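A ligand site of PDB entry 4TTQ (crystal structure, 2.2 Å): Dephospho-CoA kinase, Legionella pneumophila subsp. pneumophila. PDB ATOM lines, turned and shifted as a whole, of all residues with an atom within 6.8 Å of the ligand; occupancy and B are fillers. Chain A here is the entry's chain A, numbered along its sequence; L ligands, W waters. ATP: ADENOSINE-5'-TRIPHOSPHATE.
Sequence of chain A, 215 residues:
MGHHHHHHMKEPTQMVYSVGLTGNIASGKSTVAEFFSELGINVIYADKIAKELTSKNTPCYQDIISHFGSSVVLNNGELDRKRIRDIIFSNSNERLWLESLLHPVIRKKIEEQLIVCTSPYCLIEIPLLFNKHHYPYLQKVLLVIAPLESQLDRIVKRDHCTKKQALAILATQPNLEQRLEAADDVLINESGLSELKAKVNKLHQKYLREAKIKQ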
ATOM      1  N   GLY A  23     -16.058   5.645 -14.504  1.00  0.00           N
ATOM      2  CA  GLY A  23     -16.741   5.732 -15.779  1.00  0.00           C
ATOM      3  C   GLY A  23     -16.045   4.909 -16.846  1.00  0.00           C
ATOM      4  O   GLY A  23     -14.831   4.681 -16.799  1.00  0.00           O
ATOM      5  N   ASN A  24     -16.817   4.465 -17.823  1.00  0.00           N
ATOM      6  CA  ASN A  24     -16.220   3.782 -18.960  1.00  0.00           C
ATOM      7  C   ASN A  24     -15.783   4.907 -19.886  1.00  0.00           C
ATOM      8  O   ASN A  24     -15.975   6.097 -19.576  1.00  0.00           O
ATOM      9  CB  ASN A  24     -17.156   2.692 -19.600  1.00  0.00           C
ATOM     10  CG  ASN A  24     -18.503   3.219 -20.119  1.00  0.00           C
ATOM     11  OD1 ASN A  24     -18.868   4.383 -20.002  1.00  0.00           O
ATOM     12  ND2 ASN A  24     -19.254   2.313 -20.733  1.00  0.00           N
ATOM     13  N   ILE A  25     -15.138   4.561 -20.982  1.00  0.00           N
ATOM     14  CA  ILE A  25     -14.456   5.563 -21.773  1.00  0.00           C
ATOM     15  C   ILE A  25     -15.481   6.498 -22.378  1.00  0.00           C
ATOM     16  O   ILE A  25     -16.560   6.058 -22.751  1.00  0.00           O
ATOM     17  CB  ILE A  25     -13.563   4.916 -22.883  1.00  0.00           C
ATOM     18  CG1 ILE A  25     -12.788   6.001 -23.638  1.00  0.00           C
ATOM     19  CG2 ILE A  25     -14.415   4.023 -23.837  1.00  0.00           C
ATOM     20  CD1 ILE A  25     -11.700   5.460 -24.533  1.00  0.00           C
ATOM     21  N   ALA A  26     -15.169   7.793 -22.415  1.00  0.00           N
ATOM     22  CA  ALA A  26     -16.068   8.754 -23.043  1.00  0.00           C
ATOM     23  C   ALA A  26     -17.507   8.650 -22.515  1.00  0.00           C
ATOM     24  O   ALA A  26     -18.449   8.857 -23.249  1.00  0.00           O
ATOM     25  CB  ALA A  26     -16.069   8.527 -24.542  1.00  0.00           C
ATOM     26  N   SER A  27     -17.649   8.302 -21.243  1.00  0.00           N
ATOM     27  CA  SER A  27     -18.977   8.201 -20.606  1.00  0.00           C
ATOM     28  C   SER A  27     -19.502   9.531 -20.127  1.00  0.00           C
ATOM     29  O   SER A  27     -20.706   9.694 -19.933  1.00  0.00           O
ATOM     30  CB  SER A  27     -18.885   7.287 -19.404  1.00  0.00           C
ATOM     31  OG  SER A  27     -18.021   7.853 -18.424  1.00  0.00           O
ATOM     32  N   GLY A  28     -18.596  10.455 -19.875  1.00  0.00           N
ATOM     33  CA  GLY A  28     -18.949  11.786 -19.452  1.00  0.00           C
ATOM     34  C   GLY A  28     -18.544  12.074 -18.012  1.00  0.00           C
ATOM     35  O   GLY A  28     -19.085  12.993 -17.391  1.00  0.00           O
ATOM     36  N   LYS A  29     -17.583  11.314 -17.474  1.00  0.00           N
ATOM     37  CA  LYS A  29     -17.457  11.304 -16.034  1.00  0.00           C
ATOM     38  C   LYS A  29     -16.818  12.585 -15.575  1.00  0.00           C
ATOM     39  O   LYS A  29     -17.128  13.083 -14.511  1.00  0.00           O
ATOM     40  CB  LYS A  29     -16.735  10.067 -15.534  1.00  0.00           C
ATOM     41  CG  LYS A  29     -15.344   9.968 -15.839  1.00  0.00           C
ATOM     42  CD  LYS A  29     -14.667   8.953 -14.918  1.00  0.00           C
ATOM     43  CE  LYS A  29     -13.215   8.641 -15.423  1.00  0.00           C
ATOM     44  NZ  LYS A  29     -13.252   7.904 -16.755  1.00  0.00           N
ATOM     45  N   SER A  30     -15.954  13.150 -16.394  1.00  0.00           N
ATOM     46  CA  SER A  30     -15.396  14.436 -16.078  1.00  0.00           C
ATOM     47  C   SER A  30     -16.474  15.482 -15.885  1.00  0.00           C
ATOM     48  O   SER A  30     -16.367  16.331 -15.020  1.00  0.00           O
ATOM     49  CB  SER A  30     -14.432  14.876 -17.162  1.00  0.00           C
ATOM     50  OG  SER A  30     -13.155  14.385 -16.855  1.00  0.00           O
ATOM     51  N   THR A  31     -17.498  15.437 -16.723  1.00  0.00           N
ATOM     52  CA  THR A  31     -18.560  16.417 -16.646  1.00  0.00           C
ATOM     53  C   THR A  31     -19.346  16.177 -15.368  1.00  0.00           C
ATOM     54  O   THR A  31     -19.815  17.119 -14.719  1.00  0.00           O
ATOM     55  CB  THR A  31     -19.452  16.317 -17.873  1.00  0.00           C
ATOM     56  OG1 THR A  31     -18.636  16.419 -19.038  1.00  0.00           O
ATOM     57  CG2 THR A  31     -20.495  17.414 -17.884  1.00  0.00           C
ATOM     58  N   VAL A  32     -19.472  14.912 -15.008  1.00  0.00           N
ATOM     59  CA  VAL A  32     -20.160  14.540 -13.810  1.00  0.00           C
ATOM     60  C   VAL A  32     -19.415  15.100 -12.640  1.00  0.00           C
ATOM     61  O   VAL A  32     -20.026  15.636 -11.728  1.00  0.00           O
ATOM     62  CB  VAL A  32     -20.290  13.008 -13.691  1.00  0.00           C
ATOM     63  CG1 VAL A  32     -20.726  12.618 -12.331  1.00  0.00           C
ATOM     64  CG2 VAL A  32     -21.317  12.508 -14.682  1.00  0.00           C
ATOM     65  N   GLU A 125     -12.401  10.577  -7.995  1.00  0.00           N
ATOM     66  CA  GLU A 125     -12.340   9.967  -9.318  1.00  0.00           C
ATOM     67  C   GLU A 125     -11.199   8.986  -9.368  1.00  0.00           C
ATOM     68  O   GLU A 125     -10.049   9.363  -9.179  1.00  0.00           O
ATOM     69  CB  GLU A 125     -12.179  11.013 -10.429  1.00  0.00           C
ATOM     70  CG  GLU A 125     -12.108  10.411 -11.832  1.00  0.00           C
ATOM     71  CD  GLU A 125     -12.310  11.426 -12.979  1.00  0.00           C
ATOM     72  OE1 GLU A 125     -11.815  11.180 -14.096  1.00  0.00           O
ATOM     73  OE2 GLU A 125     -12.955  12.464 -12.776  1.00  0.00           O
ATOM     74  N   ARG A 154     -18.272  10.510 -29.365  1.00  0.00           N
ATOM     75  CA  ARG A 154     -17.347  11.204 -28.506  1.00  0.00           C
ATOM     76  C   ARG A 154     -15.913  10.848 -28.892  1.00  0.00           C
ATOM     77  O   ARG A 154     -15.065  11.717 -29.020  1.00  0.00           O
ATOM     78  CB  ARG A 154     -17.640  10.859 -27.039  1.00  0.00           C
ATOM     79  CG  ARG A 154     -17.469  12.023 -26.063  1.00  0.00           C
ATOM     80  CD  ARG A 154     -18.818  12.488 -25.496  1.00  0.00           C
ATOM     81  NE  ARG A 154     -19.399  11.498 -24.595  1.00  0.00           N
ATOM     82  CZ  ARG A 154     -20.683  11.414 -24.302  1.00  0.00           C
ATOM     83  NH1 ARG A 154     -21.548  12.280 -24.827  1.00  0.00           N
ATOM     84  NH2 ARG A 154     -21.101  10.486 -23.473  1.00  0.00           N
ATOM     85  N   ILE A 155     -15.629   9.571 -29.109  1.00  0.00           N
ATOM     86  CA  ILE A 155     -14.259   9.162 -29.407  1.00  0.00           C
ATOM     87  C   ILE A 155     -13.819   9.705 -30.762  1.00  0.00           C
ATOM     88  O   ILE A 155     -12.646   9.998 -30.985  1.00  0.00           O
ATOM     89  CB  ILE A 155     -14.114   7.642 -29.412  1.00  0.00           C
ATOM     90  CG1 ILE A 155     -14.251   7.132 -27.983  1.00  0.00           C
ATOM     91  CG2 ILE A 155     -12.730   7.212 -29.977  1.00  0.00           C
ATOM     92  CD1 ILE A 155     -14.303   5.638 -27.870  1.00  0.00           C
ATOM     93  N   LYS A 157     -14.821  12.582 -32.162  1.00  0.00           N
ATOM     94  CA  LYS A 157     -14.505  14.023 -32.044  1.00  0.00           C
ATOM     95  C   LYS A 157     -13.152  14.243 -31.363  1.00  0.00           C
ATOM     96  O   LYS A 157     -12.480  15.245 -31.600  1.00  0.00           O
ATOM     97  CB  LYS A 157     -15.586  14.758 -31.264  1.00  0.00           C
ATOM     98  CG  LYS A 157     -15.687  14.325 -29.808  1.00  0.00           C
ATOM     99  CD  LYS A 157     -16.496  15.251 -28.894  1.00  0.00           C
ATOM    100  CE  LYS A 157     -16.064  15.077 -27.449  1.00  0.00           C
ATOM    101  NZ  LYS A 157     -14.734  15.645 -27.205  1.00  0.00           N
ATOM    102  N   ARG A 158     -12.775  13.297 -30.513  1.00  0.00           N
ATOM    103  CA  ARG A 158     -11.608  13.434 -29.642  1.00  0.00           C
ATOM    104  C   ARG A 158     -10.358  12.753 -30.186  1.00  0.00           C
ATOM    105  O   ARG A 158      -9.247  13.134 -29.853  1.00  0.00           O
ATOM    106  CB  ARG A 158     -11.938  12.832 -28.265  1.00  0.00           C
ATOM    107  CG  ARG A 158     -10.982  13.213 -27.154  1.00  0.00           C
ATOM    108  CD  ARG A 158     -11.377  12.514 -25.859  1.00  0.00           C
ATOM    109  NE  ARG A 158     -11.535  13.454 -24.745  1.00  0.00           N
ATOM    110  CZ  ARG A 158     -12.679  13.734 -24.098  1.00  0.00           C
ATOM    111  NH1 ARG A 158     -13.831  13.152 -24.439  1.00  0.00           N
ATOM    112  NH2 ARG A 158     -12.665  14.603 -23.105  1.00  0.00           N
ATOM    113  N   ASN A 189     -25.644   7.960 -18.823  1.00  0.00           N
ATOM    114  CA  ASN A 189     -25.541   9.258 -19.449  1.00  0.00           C
ATOM    115  C   ASN A 189     -25.992   9.164 -20.862  1.00  0.00           C
ATOM    116  O   ASN A 189     -25.186   8.971 -21.771  1.00  0.00           O
ATOM    117  CB  ASN A 189     -24.106   9.776 -19.397  1.00  0.00           C
ATOM    118  CG  ASN A 189     -23.966  11.159 -20.018  1.00  0.00           C
ATOM    119  OD1 ASN A 189     -24.947  11.878 -20.148  1.00  0.00           O
ATOM    120  ND2 ASN A 189     -22.743  11.541 -20.380  1.00  0.00           N
ATOM    121  N   GLU A 190     -27.308   9.308 -21.049  1.00  0.00           N
ATOM    122  CA  GLU A 190     -27.905   8.903 -22.311  1.00  0.00           C
ATOM    123  C   GLU A 190     -28.814   9.952 -22.913  1.00  0.00           C
ATOM    124  O   GLU A 190     -29.347   9.733 -23.981  1.00  0.00           O
ATOM    125  CB  GLU A 190     -28.670   7.578 -22.153  1.00  0.00           C
ATOM    126  CG  GLU A 190     -29.943   7.664 -21.299  1.00  0.00           C
ATOM    127  CD  GLU A 190     -30.712   6.335 -21.181  1.00  0.00           C
ATOM    128  OE1 GLU A 190     -31.507   6.221 -20.217  1.00  0.00           O
ATOM    129  OE2 GLU A 190     -30.572   5.433 -22.041  1.00  0.00           O
ATOM    130  N   SER A 191     -28.980  11.105 -22.255  1.00  0.00           N
ATOM    131  CA  SER A 191     -29.698  12.214 -22.886  1.00  0.00           C
ATOM    132  C   SER A 191     -28.681  13.352 -23.003  1.00  0.00           C
ATOM    133  O   SER A 191     -27.576  13.116 -23.431  1.00  0.00           O
ATOM    134  CB  SER A 191     -30.951  12.628 -22.102  1.00  0.00           C
ATOM    135  OG  SER A 191     -31.484  11.544 -21.352  1.00  0.00           O
ATOM    136  N   GLY A 192     -29.054  14.572 -22.625  1.00  0.00           N
ATOM    137  CA  GLY A 192     -28.168  15.709 -22.755  1.00  0.00           C
ATOM    138  C   GLY A 192     -27.520  16.106 -21.432  1.00  0.00           C
ATOM    139  O   GLY A 192     -27.694  15.463 -20.414  1.00  0.00           O
ATOM    140  N   LEU A 193     -26.760  17.179 -21.489  1.00  0.00           N
ATOM    141  CA  LEU A 193     -26.110  17.706 -20.302  1.00  0.00           C
ATOM    142  C   LEU A 193     -27.128  18.029 -19.243  1.00  0.00           C
ATOM    143  O   LEU A 193     -26.880  17.858 -18.056  1.00  0.00           O
ATOM    144  CB  LEU A 193     -25.322  18.960 -20.658  1.00  0.00           C
ATOM    145  CG  LEU A 193     -24.067  18.618 -21.428  1.00  0.00           C
ATOM    146  CD1 LEU A 193     -23.411  19.898 -21.900  1.00  0.00           C
ATOM    147  CD2 LEU A 193     -23.086  17.823 -20.572  1.00  0.00           C
ATOM    148  N   SER A 194     -28.270  18.511 -19.677  1.00  0.00           N
ATOM    149  CA  SER A 194     -29.298  18.932 -18.760  1.00  0.00           C
ATOM    150  C   SER A 194     -29.801  17.719 -17.937  1.00  0.00           C
ATOM    151  O   SER A 194     -29.914  17.799 -16.720  1.00  0.00           O
ATOM    152  CB  SER A 194     -30.427  19.602 -19.535  1.00  0.00           C
ATOM    153  OG  SER A 194     -31.443  20.082 -18.714  1.00  0.00           O
ATOM    154  N   GLU A 195     -30.061  16.594 -18.581  1.00  0.00           N
ATOM    155  CA  GLU A 195     -30.523  15.461 -17.817  1.00  0.00           C
ATOM    156  C   GLU A 195     -29.362  14.954 -16.961  1.00  0.00           C
ATOM    157  O   GLU A 195     -29.556  14.372 -15.884  1.00  0.00           O
ATOM    158  CB  GLU A 195     -31.076  14.377 -18.769  1.00  0.00           C
ATOM    159  CG  GLU A 195     -32.289  14.831 -19.647  1.00  0.00           C
ATOM    160  CD  GLU A 195     -31.917  15.667 -20.916  1.00  0.00           C
ATOM    161  OE1 GLU A 195     -30.713  15.890 -21.214  1.00  0.00           O
ATOM    162  OE2 GLU A 195     -32.854  16.099 -21.630  1.00  0.00           O
ATOM    163  N   LEU A 196     -28.153  15.140 -17.439  1.00  0.00           N
ATOM    164  CA  LEU A 196     -27.005  14.679 -16.692  1.00  0.00           C
ATOM    165  C   LEU A 196     -26.910  15.444 -15.356  1.00  0.00           C
ATOM    166  O   LEU A 196     -26.771  14.853 -14.275  1.00  0.00           O
ATOM    167  CB  LEU A 196     -25.754  14.839 -17.522  1.00  0.00           C
ATOM    168  CG  LEU A 196     -24.516  14.327 -16.841  1.00  0.00           C
ATOM    169  CD1 LEU A 196     -24.644  12.828 -16.639  1.00  0.00           C
ATOM    170  CD2 LEU A 196     -23.286  14.647 -17.667  1.00  0.00           C
HETATM  171  PG  ATP L   1     -12.701  10.097 -20.632  1.00  0.00           P
HETATM  172  O1G ATP L   1     -11.279  10.380 -20.166  1.00  0.00           O
HETATM  173  O2G ATP L   1     -12.913   9.572 -22.047  1.00  0.00           O
HETATM  174  O3G ATP L   1     -13.553   9.358 -19.604  1.00  0.00           O
HETATM  175  PB  ATP L   1     -14.866  11.844 -20.042  1.00  0.00           P
HETATM  176  O1B ATP L   1     -15.829  10.868 -20.600  1.00  0.00           O
HETATM  177  O2B ATP L   1     -14.737  11.868 -18.555  1.00  0.00           O
HETATM  178  O3B ATP L   1     -13.413  11.540 -20.732  1.00  0.00           O
HETATM  179  PA  ATP L   1     -16.428  14.036 -20.768  1.00  0.00           P
HETATM  180  O1A ATP L   1     -16.936  12.929 -21.643  1.00  0.00           O
HETATM  181  O2A ATP L   1     -16.969  14.460 -19.416  1.00  0.00           O
HETATM  182  O3A ATP L   1     -15.003  13.404 -20.481  1.00  0.00           O
HETATM  183  O5' ATP L   1     -16.442  15.260 -21.818  1.00  0.00           O
HETATM  184  C5' ATP L   1     -16.733  15.027 -23.216  1.00  0.00           C
HETATM  185  C4' ATP L   1     -17.569  16.138 -23.841  1.00  0.00           C
HETATM  186  O4' ATP L   1     -18.869  15.573 -23.986  1.00  0.00           O
HETATM  187  C3' ATP L   1     -17.736  17.461 -23.062  1.00  0.00           C
HETATM  188  O3' ATP L   1     -17.676  18.571 -23.979  1.00  0.00           O
HETATM  189  C2' ATP L   1     -19.117  17.346 -22.445  1.00  0.00           C
HETATM  190  O2' ATP L   1     -19.764  18.593 -22.155  1.00  0.00           O
HETATM  191  C1' ATP L   1     -19.820  16.520 -23.511  1.00  0.00           C
HETATM  192  N9  ATP L   1     -20.945  15.781 -22.965  1.00  0.00           N
HETATM  193  C8  ATP L   1     -20.893  14.964 -21.895  1.00  0.00           C
HETATM  194  N7  ATP L   1     -22.105  14.424 -21.659  1.00  0.00           N
HETATM  195  C5  ATP L   1     -22.919  14.914 -22.615  1.00  0.00           C
HETATM  196  C6  ATP L   1     -24.330  14.723 -22.933  1.00  0.00           C
HETATM  197  N6  ATP L   1     -24.963  13.881 -22.070  1.00  0.00           N
HETATM  198  N1  ATP L   1     -24.841  15.392 -23.995  1.00  0.00           N
HETATM  199  C2  ATP L   1     -24.074  16.201 -24.754  1.00  0.00           C
HETATM  200  N3  ATP L   1     -22.768  16.416 -24.509  1.00  0.00           N
HETATM  201  C4  ATP L   1     -22.160  15.802 -23.469  1.00  0.00           C
HETATM  202  O   HOH W   1     -11.815   6.593 -19.952  1.00  0.00           O
HETATM  203  O   HOH W   2      -9.963   8.475 -18.629  1.00  0.00           O
HETATM  204  O   HOH W   3     -27.354  12.569 -20.054  1.00  0.00           O
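N of Thr 31 lies within hydrogen-bond range of O2A of the ligand (2.9 Å).
OG1 of Thr 31 is in hydrogen-bond range of O2A of the ligand (2.6 Å).
The side-chain amide oxygen (OD1) of Asn 189 is in hydrogen-bond range of a nitrogen (N6) of the ligand, 2.8 Å away.
N of Ser 30 is in hydrogen-bond range of O2B of the ligand (2.8 Å).
OG of Ser 30 sits close to O2B of the ligand, at 3.4 Å.
The backbone NH (N) of Gly 28 sits at hydrogen-bond distance from an oxygen (O1B) of the ligand (2.9 Å).
The backbone NH (N) of Ala 26 sits at hydrogen-bond distance from an oxygen (O2G) of the ligand (2.9 Å).
O of Ser 191 is in hydrogen-bond range of N6 of the ligand, at 3.0 Å.
N of Lys 29 sits at hydrogen-bond distance from O2B of the ligand (3.1 Å).
NZ of Lys 29 is in salt-bridge range of O3G of the ligand (3.2 Å).
An oxygen (O1B) of the ligand is in hydrogen-bond range of the backbone NH (N) of Ser 27.
ND2 of Asn 189 is in hydrogen-bond range of O of Ser 27 (2.8 Å).
The backbone carbonyl oxygen (O) of Ala 26 sits at hydrogen-bond distance from the guanidinium group (NE) of Arg 154.
The side-chain hydroxyl (OG) of Ser 27 lies within hydrogen-bond range of the backbone carbonyl oxygen (O) of Asn 24 (2.9 Å).
The backbone NH (N) of Gly 192 sits at hydrogen-bond distance from the side-chain carboxylate (OE1) of Glu 195 (2.5 Å).
Ile 25 touches the ligand (CG1 to O2G, 3.9 Å).
Arg 154 touches the ligand (CD to O4', 3.4 Å).
Arg 158 touches the ligand.
C of Gly 192 touches N6 of the ligand, at 3.4 Å.
Leu 193 touches the ligand (CD2 to C5, 3.6 Å).
Of the 23 residues printed, 13 come within 4 Å of the ligand.
The nearest printed residue that does not touch the ligand is Lys 157 (4.1 Å).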
